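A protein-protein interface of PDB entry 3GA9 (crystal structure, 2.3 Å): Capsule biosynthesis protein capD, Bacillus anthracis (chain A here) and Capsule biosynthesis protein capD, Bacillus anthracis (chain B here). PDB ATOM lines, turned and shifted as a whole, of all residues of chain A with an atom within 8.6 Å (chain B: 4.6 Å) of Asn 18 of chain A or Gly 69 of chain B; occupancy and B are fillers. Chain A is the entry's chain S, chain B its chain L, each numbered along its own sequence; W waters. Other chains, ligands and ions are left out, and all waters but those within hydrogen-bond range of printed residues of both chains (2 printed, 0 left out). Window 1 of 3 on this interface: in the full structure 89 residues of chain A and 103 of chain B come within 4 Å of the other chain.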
ATOM      1  N   THR A   1     -21.582   2.783 -14.152  1.00  0.00           N
ATOM      2  CA  THR A   1     -22.179   4.127 -14.301  1.00  0.00           C
ATOM      3  C   THR A   1     -21.142   5.170 -13.976  1.00  0.00           C
ATOM      4  O   THR A   1     -20.260   4.970 -13.133  1.00  0.00           O
ATOM      5  CB  THR A   1     -23.410   4.268 -13.380  1.00  0.00           C
ATOM      6  OG1 THR A   1     -24.187   3.105 -13.575  1.00  0.00           O
ATOM      7  CG2 THR A   1     -24.254   5.460 -13.760  1.00  0.00           C
ATOM      8  N   THR A   2     -21.263   6.300 -14.638  1.00  0.00           N
ATOM      9  CA  THR A   2     -20.288   7.335 -14.483  1.00  0.00           C
ATOM     10  C   THR A   2     -20.984   8.641 -14.748  1.00  0.00           C
ATOM     11  O   THR A   2     -21.906   8.725 -15.572  1.00  0.00           O
ATOM     12  CB  THR A   2     -19.043   7.115 -15.425  1.00  0.00           C
ATOM     13  OG1 THR A   2     -17.951   7.928 -14.963  1.00  0.00           O
ATOM     14  CG2 THR A   2     -19.371   7.503 -16.878  1.00  0.00           C
ATOM     15  N   HIS A   3     -20.575   9.652 -14.004  1.00  0.00           N
ATOM     16  CA  HIS A   3     -21.179  10.941 -14.160  1.00  0.00           C
ATOM     17  C   HIS A   3     -20.109  11.980 -14.357  1.00  0.00           C
ATOM     18  O   HIS A   3     -19.084  11.924 -13.682  1.00  0.00           O
ATOM     19  CB  HIS A   3     -22.036  11.352 -12.927  1.00  0.00           C
ATOM     20  CG  HIS A   3     -22.881  12.534 -13.232  1.00  0.00           C
ATOM     21  ND1 HIS A   3     -22.470  13.823 -12.972  1.00  0.00           N
ATOM     22  CD2 HIS A   3     -24.031  12.636 -13.932  1.00  0.00           C
ATOM     23  CE1 HIS A   3     -23.361  14.669 -13.457  1.00  0.00           C
ATOM     24  NE2 HIS A   3     -24.322  13.975 -14.040  1.00  0.00           N
ATOM     25  N   PHE A   4     -20.356  12.953 -15.219  1.00  0.00           N
ATOM     26  CA  PHE A   4     -19.404  14.035 -15.353  1.00  0.00           C
ATOM     27  C   PHE A   4     -20.112  15.357 -15.637  1.00  0.00           C
ATOM     28  O   PHE A   4     -21.257  15.390 -16.033  1.00  0.00           O
ATOM     29  CB  PHE A   4     -18.315  13.701 -16.436  1.00  0.00           C
ATOM     30  CG  PHE A   4     -18.846  13.744 -17.829  1.00  0.00           C
ATOM     31  CD1 PHE A   4     -19.254  12.571 -18.470  1.00  0.00           C
ATOM     32  CD2 PHE A   4     -18.993  14.964 -18.492  1.00  0.00           C
ATOM     33  CE1 PHE A   4     -19.797  12.605 -19.738  1.00  0.00           C
ATOM     34  CE2 PHE A   4     -19.521  15.028 -19.777  1.00  0.00           C
ATOM     35  CZ  PHE A   4     -19.928  13.858 -20.401  1.00  0.00           C
ATOM     36  N   SER A  15     -24.270  18.088 -17.918  1.00  0.00           N
ATOM     37  CA  SER A  15     -24.261  17.176 -16.792  1.00  0.00           C
ATOM     38  C   SER A  15     -24.797  15.861 -17.310  1.00  0.00           C
ATOM     39  O   SER A  15     -25.925  15.788 -17.805  1.00  0.00           O
ATOM     40  CB  SER A  15     -25.117  17.724 -15.646  1.00  0.00           C
ATOM     41  OG  SER A  15     -25.092  16.828 -14.543  1.00  0.00           O
ATOM     42  N   SER A  16     -23.981  14.825 -17.223  1.00  0.00           N
ATOM     43  CA  SER A  16     -24.216  13.647 -18.006  1.00  0.00           C
ATOM     44  C   SER A  16     -23.795  12.423 -17.247  1.00  0.00           C
ATOM     45  O   SER A  16     -22.754  12.419 -16.568  1.00  0.00           O
ATOM     46  CB  SER A  16     -23.422  13.705 -19.328  1.00  0.00           C
ATOM     47  OG  SER A  16     -23.682  12.566 -20.136  1.00  0.00           O
ATOM     48  N   THR A  17     -24.622  11.387 -17.369  1.00  0.00           N
ATOM     49  CA  THR A  17     -24.346  10.100 -16.755  1.00  0.00           C
ATOM     50  C   THR A  17     -24.594   9.000 -17.760  1.00  0.00           C
ATOM     51  O   THR A  17     -25.632   9.003 -18.455  1.00  0.00           O
ATOM     52  CB  THR A  17     -25.027   9.913 -15.324  1.00  0.00           C
ATOM     53  OG1 THR A  17     -25.260   8.527 -15.031  1.00  0.00           O
ATOM     54  CG2 THR A  17     -26.223  10.672 -15.165  1.00  0.00           C
ATOM     55  N   ASN A  18     -23.564   8.151 -17.917  1.00  0.00           N
ATOM     56  CA  ASN A  18     -23.525   7.035 -18.879  1.00  0.00           C
ATOM     57  C   ASN A  18     -23.288   5.752 -18.127  1.00  0.00           C
ATOM     58  O   ASN A  18     -22.755   5.790 -17.030  1.00  0.00           O
ATOM     59  CB  ASN A  18     -22.388   7.217 -19.868  1.00  0.00           C
ATOM     60  CG  ASN A  18     -22.553   8.457 -20.721  1.00  0.00           C
ATOM     61  OD1 ASN A  18     -23.668   8.901 -20.978  1.00  0.00           O
ATOM     62  ND2 ASN A  18     -21.437   9.030 -21.157  1.00  0.00           N
ATOM     63  N   THR A  19     -23.634   4.620 -18.731  1.00  0.00           N
ATOM     64  CA  THR A  19     -23.675   3.379 -18.013  1.00  0.00           C
ATOM     65  C   THR A  19     -23.870   2.142 -18.872  1.00  0.00           C
ATOM     66  O   THR A  19     -24.394   2.210 -20.000  1.00  0.00           O
ATOM     67  CB  THR A  19     -24.859   3.392 -16.960  1.00  0.00           C
ATOM     68  OG1 THR A  19     -24.671   2.308 -16.021  1.00  0.00           O
ATOM     69  CG2 THR A  19     -26.250   3.299 -17.632  1.00  0.00           C
ATOM     70  N   LEU A  20     -23.499   1.013 -18.269  1.00  0.00           N
ATOM     71  CA  LEU A  20     -23.700  -0.341 -18.775  1.00  0.00           C
ATOM     72  C   LEU A  20     -24.718  -1.070 -17.875  1.00  0.00           C
ATOM     73  O   LEU A  20     -25.022  -2.227 -18.096  1.00  0.00           O
ATOM     74  CB  LEU A  20     -22.365  -1.094 -18.724  1.00  0.00           C
ATOM     75  CG  LEU A  20     -21.300  -0.654 -19.744  1.00  0.00           C
ATOM     76  CD1 LEU A  20     -19.872  -1.252 -19.435  1.00  0.00           C
ATOM     77  CD2 LEU A  20     -21.756  -1.024 -21.132  1.00  0.00           C
ATOM     78  N   SER A  21     -25.223  -0.359 -16.870  1.00  0.00           N
ATOM     79  CA  SER A  21     -25.995  -0.909 -15.743  1.00  0.00           C
ATOM     80  C   SER A  21     -25.075  -1.623 -14.796  1.00  0.00           C
ATOM     81  O   SER A  21     -24.506  -0.945 -13.961  1.00  0.00           O
ATOM     82  CB  SER A  21     -27.195  -1.731 -16.178  1.00  0.00           C
ATOM     83  OG  SER A  21     -28.041  -0.847 -16.895  1.00  0.00           O
ATOM     84  N   ASN A  22     -24.880  -2.941 -14.896  1.00  0.00           N
ATOM     85  CA  ASN A  22     -23.812  -3.553 -14.104  1.00  0.00           C
ATOM     86  C   ASN A  22     -22.428  -3.061 -14.564  1.00  0.00           C
ATOM     87  O   ASN A  22     -22.254  -2.640 -15.704  1.00  0.00           O
ATOM     88  CB  ASN A  22     -23.750  -5.074 -14.263  1.00  0.00           C
ATOM     89  CG  ASN A  22     -24.944  -5.798 -13.708  1.00  0.00           C
ATOM     90  OD1 ASN A  22     -25.674  -5.303 -12.822  1.00  0.00           O
ATOM     91  ND2 ASN A  22     -25.164  -7.013 -14.239  1.00  0.00           N
ATOM     92  N   ARG A  55     -37.345   1.960 -23.233  1.00  0.00           N
ATOM     93  CA  ARG A  55     -36.243   2.114 -22.261  1.00  0.00           C
ATOM     94  C   ARG A  55     -36.739   1.731 -20.878  1.00  0.00           C
ATOM     95  O   ARG A  55     -37.893   1.985 -20.544  1.00  0.00           O
ATOM     96  CB  ARG A  55     -35.748   3.569 -22.225  1.00  0.00           C
ATOM     97  CG  ARG A  55     -35.212   4.062 -23.533  1.00  0.00           C
ATOM     98  CD  ARG A  55     -35.482   5.548 -23.746  1.00  0.00           C
ATOM     99  NE  ARG A  55     -34.521   6.056 -24.724  1.00  0.00           N
ATOM    100  CZ  ARG A  55     -34.581   5.863 -26.046  1.00  0.00           C
ATOM    101  NH1 ARG A  55     -35.586   5.230 -26.604  1.00  0.00           N
ATOM    102  NH2 ARG A  55     -33.628   6.337 -26.823  1.00  0.00           N
ATOM    103  N   THR A  58     -34.607   4.112 -14.657  1.00  0.00           N
ATOM    104  CA  THR A  58     -33.299   4.156 -14.085  1.00  0.00           C
ATOM    105  C   THR A  58     -33.404   5.179 -13.006  1.00  0.00           C
ATOM    106  O   THR A  58     -34.254   6.076 -13.071  1.00  0.00           O
ATOM    107  CB  THR A  58     -32.207   4.577 -15.112  1.00  0.00           C
ATOM    108  OG1 THR A  58     -31.044   5.006 -14.397  1.00  0.00           O
ATOM    109  CG2 THR A  58     -32.708   5.733 -16.007  1.00  0.00           C
ATOM    110  N   MET A  60     -30.876   7.121 -12.431  1.00  0.00           N
ATOM    111  CA  MET A  60     -29.913   8.164 -12.776  1.00  0.00           C
ATOM    112  C   MET A  60     -30.577   9.552 -12.774  1.00  0.00           C
ATOM    113  O   MET A  60     -31.774   9.679 -13.121  1.00  0.00           O
ATOM    114  CB  MET A  60     -29.276   7.863 -14.139  1.00  0.00           C
ATOM    115  CG  MET A  60     -28.355   6.616 -14.198  1.00  0.00           C
ATOM    116  SD  MET A  60     -27.590   6.421 -16.057  1.00  0.00           S
ATOM    117  CE  MET A  60     -29.031   5.351 -16.925  1.00  0.00           C
ATOM    118  N   PRO A  62     -28.857  13.236 -13.818  1.00  0.00           N
ATOM    119  CA  PRO A  62     -28.008  14.380 -14.085  1.00  0.00           C
ATOM    120  C   PRO A  62     -28.768  15.662 -13.769  1.00  0.00           C
ATOM    121  O   PRO A  62     -29.881  15.814 -14.231  1.00  0.00           O
ATOM    122  CB  PRO A  62     -27.789  14.326 -15.603  1.00  0.00           C
ATOM    123  CG  PRO A  62     -28.185  13.020 -16.035  1.00  0.00           C
ATOM    124  CD  PRO A  62     -29.007  12.354 -14.986  1.00  0.00           C
ATOM    125  N   SER A  76     -24.251  11.525 -10.081  1.00  0.00           N
ATOM    126  CA  SER A  76     -23.525  10.431  -9.398  1.00  0.00           C
ATOM    127  C   SER A  76     -24.019   9.073  -9.900  1.00  0.00           C
ATOM    128  O   SER A  76     -25.150   8.978 -10.304  1.00  0.00           O
ATOM    129  CB  SER A  76     -23.713  10.535  -7.884  1.00  0.00           C
ATOM    130  OG  SER A  76     -23.136   9.441  -7.205  1.00  0.00           O
ATOM    131  N   PRO A  77     -23.144   8.045  -9.959  1.00  0.00           N
ATOM    132  CA  PRO A  77     -23.653   6.658 -10.133  1.00  0.00           C
ATOM    133  C   PRO A  77     -24.146   6.138  -8.804  1.00  0.00           C
ATOM    134  O   PRO A  77     -24.075   6.850  -7.777  1.00  0.00           O
ATOM    135  CB  PRO A  77     -22.387   5.866 -10.492  1.00  0.00           C
ATOM    136  CG  PRO A  77     -21.299   6.644  -9.724  1.00  0.00           C
ATOM    137  CD  PRO A  77     -21.671   8.083 -10.028  1.00  0.00           C
ATOM    138  N   GLY A  78     -24.579   4.886  -8.825  1.00  0.00           N
ATOM    139  CA  GLY A  78     -24.925   4.153  -7.621  1.00  0.00           C
ATOM    140  C   GLY A  78     -26.344   3.606  -7.586  1.00  0.00           C
ATOM    141  O   GLY A  78     -26.883   3.414  -6.510  1.00  0.00           O
ATOM    142  N   ARG A 169     -14.196   6.795  -6.288  1.00  0.00           N
ATOM    143  CA  ARG A 169     -13.995   6.184  -7.613  1.00  0.00           C
ATOM    144  C   ARG A 169     -12.821   6.833  -8.318  1.00  0.00           C
ATOM    145  O   ARG A 169     -12.784   6.897  -9.555  1.00  0.00           O
ATOM    146  CB  ARG A 169     -15.250   6.257  -8.483  1.00  0.00           C
ATOM    147  CG  ARG A 169     -16.490   5.721  -7.811  1.00  0.00           C
ATOM    148  CD  ARG A 169     -17.544   5.344  -8.789  1.00  0.00           C
ATOM    149  NE  ARG A 169     -18.691   4.740  -8.118  1.00  0.00           N
ATOM    150  CZ  ARG A 169     -19.627   4.011  -8.730  1.00  0.00           C
ATOM    151  NH1 ARG A 169     -19.569   3.807 -10.047  1.00  0.00           N
ATOM    152  NH2 ARG A 169     -20.660   3.541  -8.034  1.00  0.00           N
ATOM    153  N   SER B  52     -16.796  11.546 -22.849  1.00  0.00           N
ATOM    154  CA  SER B  52     -17.614  10.339 -22.782  1.00  0.00           C
ATOM    155  C   SER B  52     -16.884   9.184 -23.435  1.00  0.00           C
ATOM    156  O   SER B  52     -16.819   8.062 -22.871  1.00  0.00           O
ATOM    157  CB  SER B  52     -18.969  10.497 -23.490  1.00  0.00           C
ATOM    158  OG  SER B  52     -19.539  11.717 -23.219  1.00  0.00           O
ATOM    159  N   ALA B  62     -17.459   0.964 -16.249  1.00  0.00           N
ATOM    160  CA  ALA B  62     -18.572   1.818 -15.835  1.00  0.00           C
ATOM    161  C   ALA B  62     -19.433   2.370 -16.962  1.00  0.00           C
ATOM    162  O   ALA B  62     -20.567   2.770 -16.734  1.00  0.00           O
ATOM    163  CB  ALA B  62     -18.043   2.976 -15.006  1.00  0.00           C
ATOM    164  N   SER B  63     -18.881   2.456 -18.166  1.00  0.00           N
ATOM    165  CA  SER B  63     -19.627   2.985 -19.306  1.00  0.00           C
ATOM    166  C   SER B  63     -18.899   2.619 -20.575  1.00  0.00           C
ATOM    167  O   SER B  63     -17.761   2.135 -20.525  1.00  0.00           O
ATOM    168  CB  SER B  63     -19.787   4.524 -19.211  1.00  0.00           C
ATOM    169  OG  SER B  63     -18.659   5.255 -19.729  1.00  0.00           O
ATOM    170  N   GLY B  68     -25.499   3.049 -22.707  1.00  0.00           N
ATOM    171  CA  GLY B  68     -26.235   4.282 -23.057  1.00  0.00           C
ATOM    172  C   GLY B  68     -26.123   5.268 -21.901  1.00  0.00           C
ATOM    173  O   GLY B  68     -25.264   5.100 -21.015  1.00  0.00           O
ATOM    174  N   GLY B  69     -26.969   6.285 -21.900  1.00  0.00           N
ATOM    175  CA  GLY B  69     -26.944   7.270 -20.848  1.00  0.00           C
ATOM    176  C   GLY B  69     -27.840   8.434 -21.189  1.00  0.00           C
ATOM    177  O   GLY B  69     -28.683   8.339 -22.087  1.00  0.00           O
ATOM    178  N   GLY B  70     -27.642   9.545 -20.478  1.00  0.00           N
ATOM    179  CA  GLY B  70     -28.387  10.764 -20.748  1.00  0.00           C
ATOM    180  C   GLY B  70     -27.594  12.018 -20.491  1.00  0.00           C
ATOM    181  O   GLY B  70     -26.720  12.050 -19.607  1.00  0.00           O
ATOM    182  N   ILE B  82     -30.934  15.095 -23.649  1.00  0.00           N
ATOM    183  CA  ILE B  82     -30.788  14.018 -24.646  1.00  0.00           C
ATOM    184  C   ILE B  82     -30.790  12.624 -23.959  1.00  0.00           C
ATOM    185  O   ILE B  82     -30.016  12.347 -23.028  1.00  0.00           O
ATOM    186  CB  ILE B  82     -29.494  14.153 -25.500  1.00  0.00           C
ATOM    187  CG1 ILE B  82     -29.038  15.614 -25.652  1.00  0.00           C
ATOM    188  CG2 ILE B  82     -29.645  13.388 -26.829  1.00  0.00           C
ATOM    189  CD1 ILE B  82     -29.814  16.404 -26.709  1.00  0.00           C
ATOM    190  N   ASP B  83     -31.665  11.755 -24.430  1.00  0.00           N
ATOM    191  CA  ASP B  83     -31.847  10.455 -23.826  1.00  0.00           C
ATOM    192  C   ASP B  83     -31.379   9.408 -24.826  1.00  0.00           C
ATOM    193  O   ASP B  83     -32.059   9.141 -25.801  1.00  0.00           O
ATOM    194  CB  ASP B  83     -33.338  10.276 -23.478  1.00  0.00           C
ATOM    195  CG  ASP B  83     -33.704   8.866 -23.110  1.00  0.00           C
ATOM    196  OD1 ASP B  83     -32.868   7.944 -23.177  1.00  0.00           O
ATOM    197  OD2 ASP B  83     -34.873   8.663 -22.727  1.00  0.00           O
ATOM    198  N   TYR B  84     -30.224   8.800 -24.554  1.00  0.00           N
ATOM    199  CA  TYR B  84     -29.666   7.768 -25.430  1.00  0.00           C
ATOM    200  C   TYR B  84     -29.502   6.454 -24.670  1.00  0.00           C
ATOM    201  O   TYR B  84     -28.527   5.724 -24.805  1.00  0.00           O
ATOM    202  CB  TYR B  84     -28.338   8.218 -26.060  1.00  0.00           C
ATOM    203  CG  TYR B  84     -27.387   8.865 -25.084  1.00  0.00           C
ATOM    204  CD1 TYR B  84     -26.426   8.110 -24.408  1.00  0.00           C
ATOM    205  CD2 TYR B  84     -27.447  10.245 -24.842  1.00  0.00           C
ATOM    206  CE1 TYR B  84     -25.539   8.728 -23.498  1.00  0.00           C
ATOM    207  CE2 TYR B  84     -26.595  10.864 -23.968  1.00  0.00           C
ATOM    208  CZ  TYR B  84     -25.638  10.109 -23.289  1.00  0.00           C
ATOM    209  OH  TYR B  84     -24.783  10.763 -22.425  1.00  0.00           O
ATOM    210  N   ARG B  85     -30.518   6.143 -23.904  1.00  0.00           N
ATOM    211  CA  ARG B  85     -30.547   4.918 -23.199  1.00  0.00           C
ATOM    212  C   ARG B  85     -30.863   3.753 -24.142  1.00  0.00           C
ATOM    213  O   ARG B  85     -31.516   3.928 -25.178  1.00  0.00           O
ATOM    214  CB  ARG B  85     -31.601   5.063 -22.126  1.00  0.00           C
ATOM    215  CG  ARG B  85     -31.518   4.071 -21.076  1.00  0.00           C
ATOM    216  CD  ARG B  85     -31.756   4.715 -19.736  1.00  0.00           C
ATOM    217  NE  ARG B  85     -32.341   3.680 -18.901  1.00  0.00           N
ATOM    218  CZ  ARG B  85     -31.636   2.779 -18.229  1.00  0.00           C
ATOM    219  NH1 ARG B  85     -30.296   2.803 -18.264  1.00  0.00           N
ATOM    220  NH2 ARG B  85     -32.285   1.864 -17.512  1.00  0.00           N
ATOM    221  N   PHE B 104     -25.426   4.758 -26.890  1.00  0.00           N
ATOM    222  CA  PHE B 104     -24.317   5.683 -26.685  1.00  0.00           C
ATOM    223  C   PHE B 104     -23.780   6.339 -27.939  1.00  0.00           C
ATOM    224  O   PHE B 104     -23.678   7.556 -27.982  1.00  0.00           O
ATOM    225  CB  PHE B 104     -23.184   4.990 -25.926  1.00  0.00           C
ATOM    226  CG  PHE B 104     -21.985   5.886 -25.650  1.00  0.00           C
ATOM    227  CD1 PHE B 104     -21.053   6.161 -26.653  1.00  0.00           C
ATOM    228  CD2 PHE B 104     -21.781   6.425 -24.388  1.00  0.00           C
ATOM    229  CE1 PHE B 104     -19.953   6.971 -26.417  1.00  0.00           C
ATOM    230  CE2 PHE B 104     -20.677   7.227 -24.127  1.00  0.00           C
ATOM    231  CZ  PHE B 104     -19.763   7.494 -25.154  1.00  0.00           C
ATOM    232  N   PHE B 240     -35.828   8.634 -16.413  1.00  0.00           N
ATOM    233  CA  PHE B 240     -34.799   8.976 -15.397  1.00  0.00           C
ATOM    234  C   PHE B 240     -35.482   9.518 -14.130  1.00  0.00           C
ATOM    235  O   PHE B 240     -36.697   9.729 -14.123  1.00  0.00           O
ATOM    236  CB  PHE B 240     -33.835  10.015 -15.956  1.00  0.00           C
ATOM    237  CG  PHE B 240     -32.932   9.491 -17.051  1.00  0.00           C
ATOM    238  CD1 PHE B 240     -31.558   9.384 -16.849  1.00  0.00           C
ATOM    239  CD2 PHE B 240     -33.447   9.108 -18.286  1.00  0.00           C
ATOM    240  CE1 PHE B 240     -30.710   8.893 -17.875  1.00  0.00           C
ATOM    241  CE2 PHE B 240     -32.616   8.633 -19.291  1.00  0.00           C
ATOM    242  CZ  PHE B 240     -31.240   8.515 -19.078  1.00  0.00           C
HETATM  243  O   HOH W   1     -18.768   7.607 -21.011  1.00  0.00           O
HETATM  244  O   HOH W   2     -22.299   4.010 -21.744  1.00  0.00           O
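The backbone carbonyl oxygen of Ala 62 of chain B lies within hydrogen-bond range of the backbone NH of Thr 1 of chain A (2.8 Å).
N of Thr 19 of chain A sits at hydrogen-bond distance from O of Gly 68 of chain B, 2.8 Å away.
The backbone carbonyl oxygen (O) of Gly 70 of chain B is in hydrogen-bond range of the side-chain hydroxyl (OG) of Ser 16 of chain A (3.1 Å).
N of Gly 70 of chain B sits at hydrogen-bond distance from O of Thr 17 of chain A (2.9 Å).
The side-chain carboxylate of Asp 83 of chain B is in salt-bridge range of the guanidinium group of Arg 55 of chain A, at 2.9 Å.
The side-chain hydroxyl (OH) of Tyr 84 of chain B sits at hydrogen-bond distance from the side-chain hydroxyl (OG) of Ser 16 of chain A.
The side-chain hydroxyl of Tyr 84 of chain B is in hydrogen-bond range of the side-chain amide oxygen of Asn 18 of chain A (2.6 Å).
Of the 12 printed residues of chain B, 11 touch a printed residue of chain A.
Hydrophobic or aromatic side chains of chain B that line the printed part of chain A: Ala 62, Tyr 84, Phe 104 and Phe 240.
Among the printed residues, 25 pairs touch across the chains.
O of Gly 69 of chain B lies within hydrogen-bond range of N of Tyr 84 of chain B, at 2.9 Å.
The side-chain hydroxyl (OG1) of Thr 1 of chain A lies within hydrogen-bond range of the side-chain hydroxyl (OG1) of Thr 19 of chain A (2.6 Å).
The backbone carbonyl oxygen (O) of Asn 18 of chain A lies within hydrogen-bond range of the backbone NH (N) of Thr 2 of chain A (2.9 Å).
NE2 of His 3 of chain A lies within hydrogen-bond range of N of Ser 16 of chain A (3.3 Å).
The backbone NH (N) of Phe 4 of chain A is in hydrogen-bond range of the backbone carbonyl oxygen (O) of Ser 16 of chain A (2.8 Å).
The side-chain hydroxyl (OG1) of Thr 58 of chain A sits at hydrogen-bond distance from the backbone NH (N) of Met 60 of chain A.
Water W1 lies within hydrogen-bond range of OG of Ser 63 of chain B (2.7 Å), O of Ser 52 of chain B (2.7 Å) and ND2 of Asn 18 of chain A (3.0 Å).
Water W2 lies within hydrogen-bond range of O of Gly 68 of chain B and O of Thr 19 of chain A.
Asn 18 of chain A touches just these residues of chain B: Ser 52, Ala 62, Ser 63, Gly 68, Gly 69, Tyr 84 and Phe 104.
Gly 69 of chain B touches two residues of chain A.
Of chain A, only Ser 16 (3.1 Å) and Asn 18 (2.6 Å) come within 4 Å of Tyr 84 of chain B.
Printed residues of chain B within 4 Å of Ser 16 of chain A: Gly 70 and Tyr 84.
Of the printed residues of chain A, Asp 83 of chain B touches Arg 55.
Arg 169 of chain A touches none of the printed residues of chain B.
The nearest residue of chain B that does not touch Asn 18 of chain A is Gly 70 of chain B (4.1 Å).
Among the printed residues, merely in contact across the chains: Met 60 of chain A with Arg 85 of chain B, Thr 17 of chain A with Gly 69 of chain B, Asn 18 of chain A with Gly 68 of chain B, Thr 19 of chain A with Ala 62 of chain B, Met 60 of chain A with Phe 240 of chain B, Asn 18 of chain A with Phe 104 of chain B, Phe 4 of chain A with Ser 52 of chain B, Thr 58 of chain A with Arg 85 of chain B, Arg 55 of chain A with Arg 85 of chain B, Asn 18 of chain A with Gly 69 of chain B, Asn 18 of chain A with Ser 52 of chain B, Thr 2 of chain A with Ser 63 of chain B, Asn 18 of chain A with Ala 62 of chain B, Leu 20 of chain A with Ala 62 of chain B, Thr 58 of chain A with Phe 240 of chain B, Asn 18 of chain A with Ser 63 of chain B, Thr 19 of chain A with Ser 63 of chain B and Pro 62 of chain A with Gly 70 of chain B.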
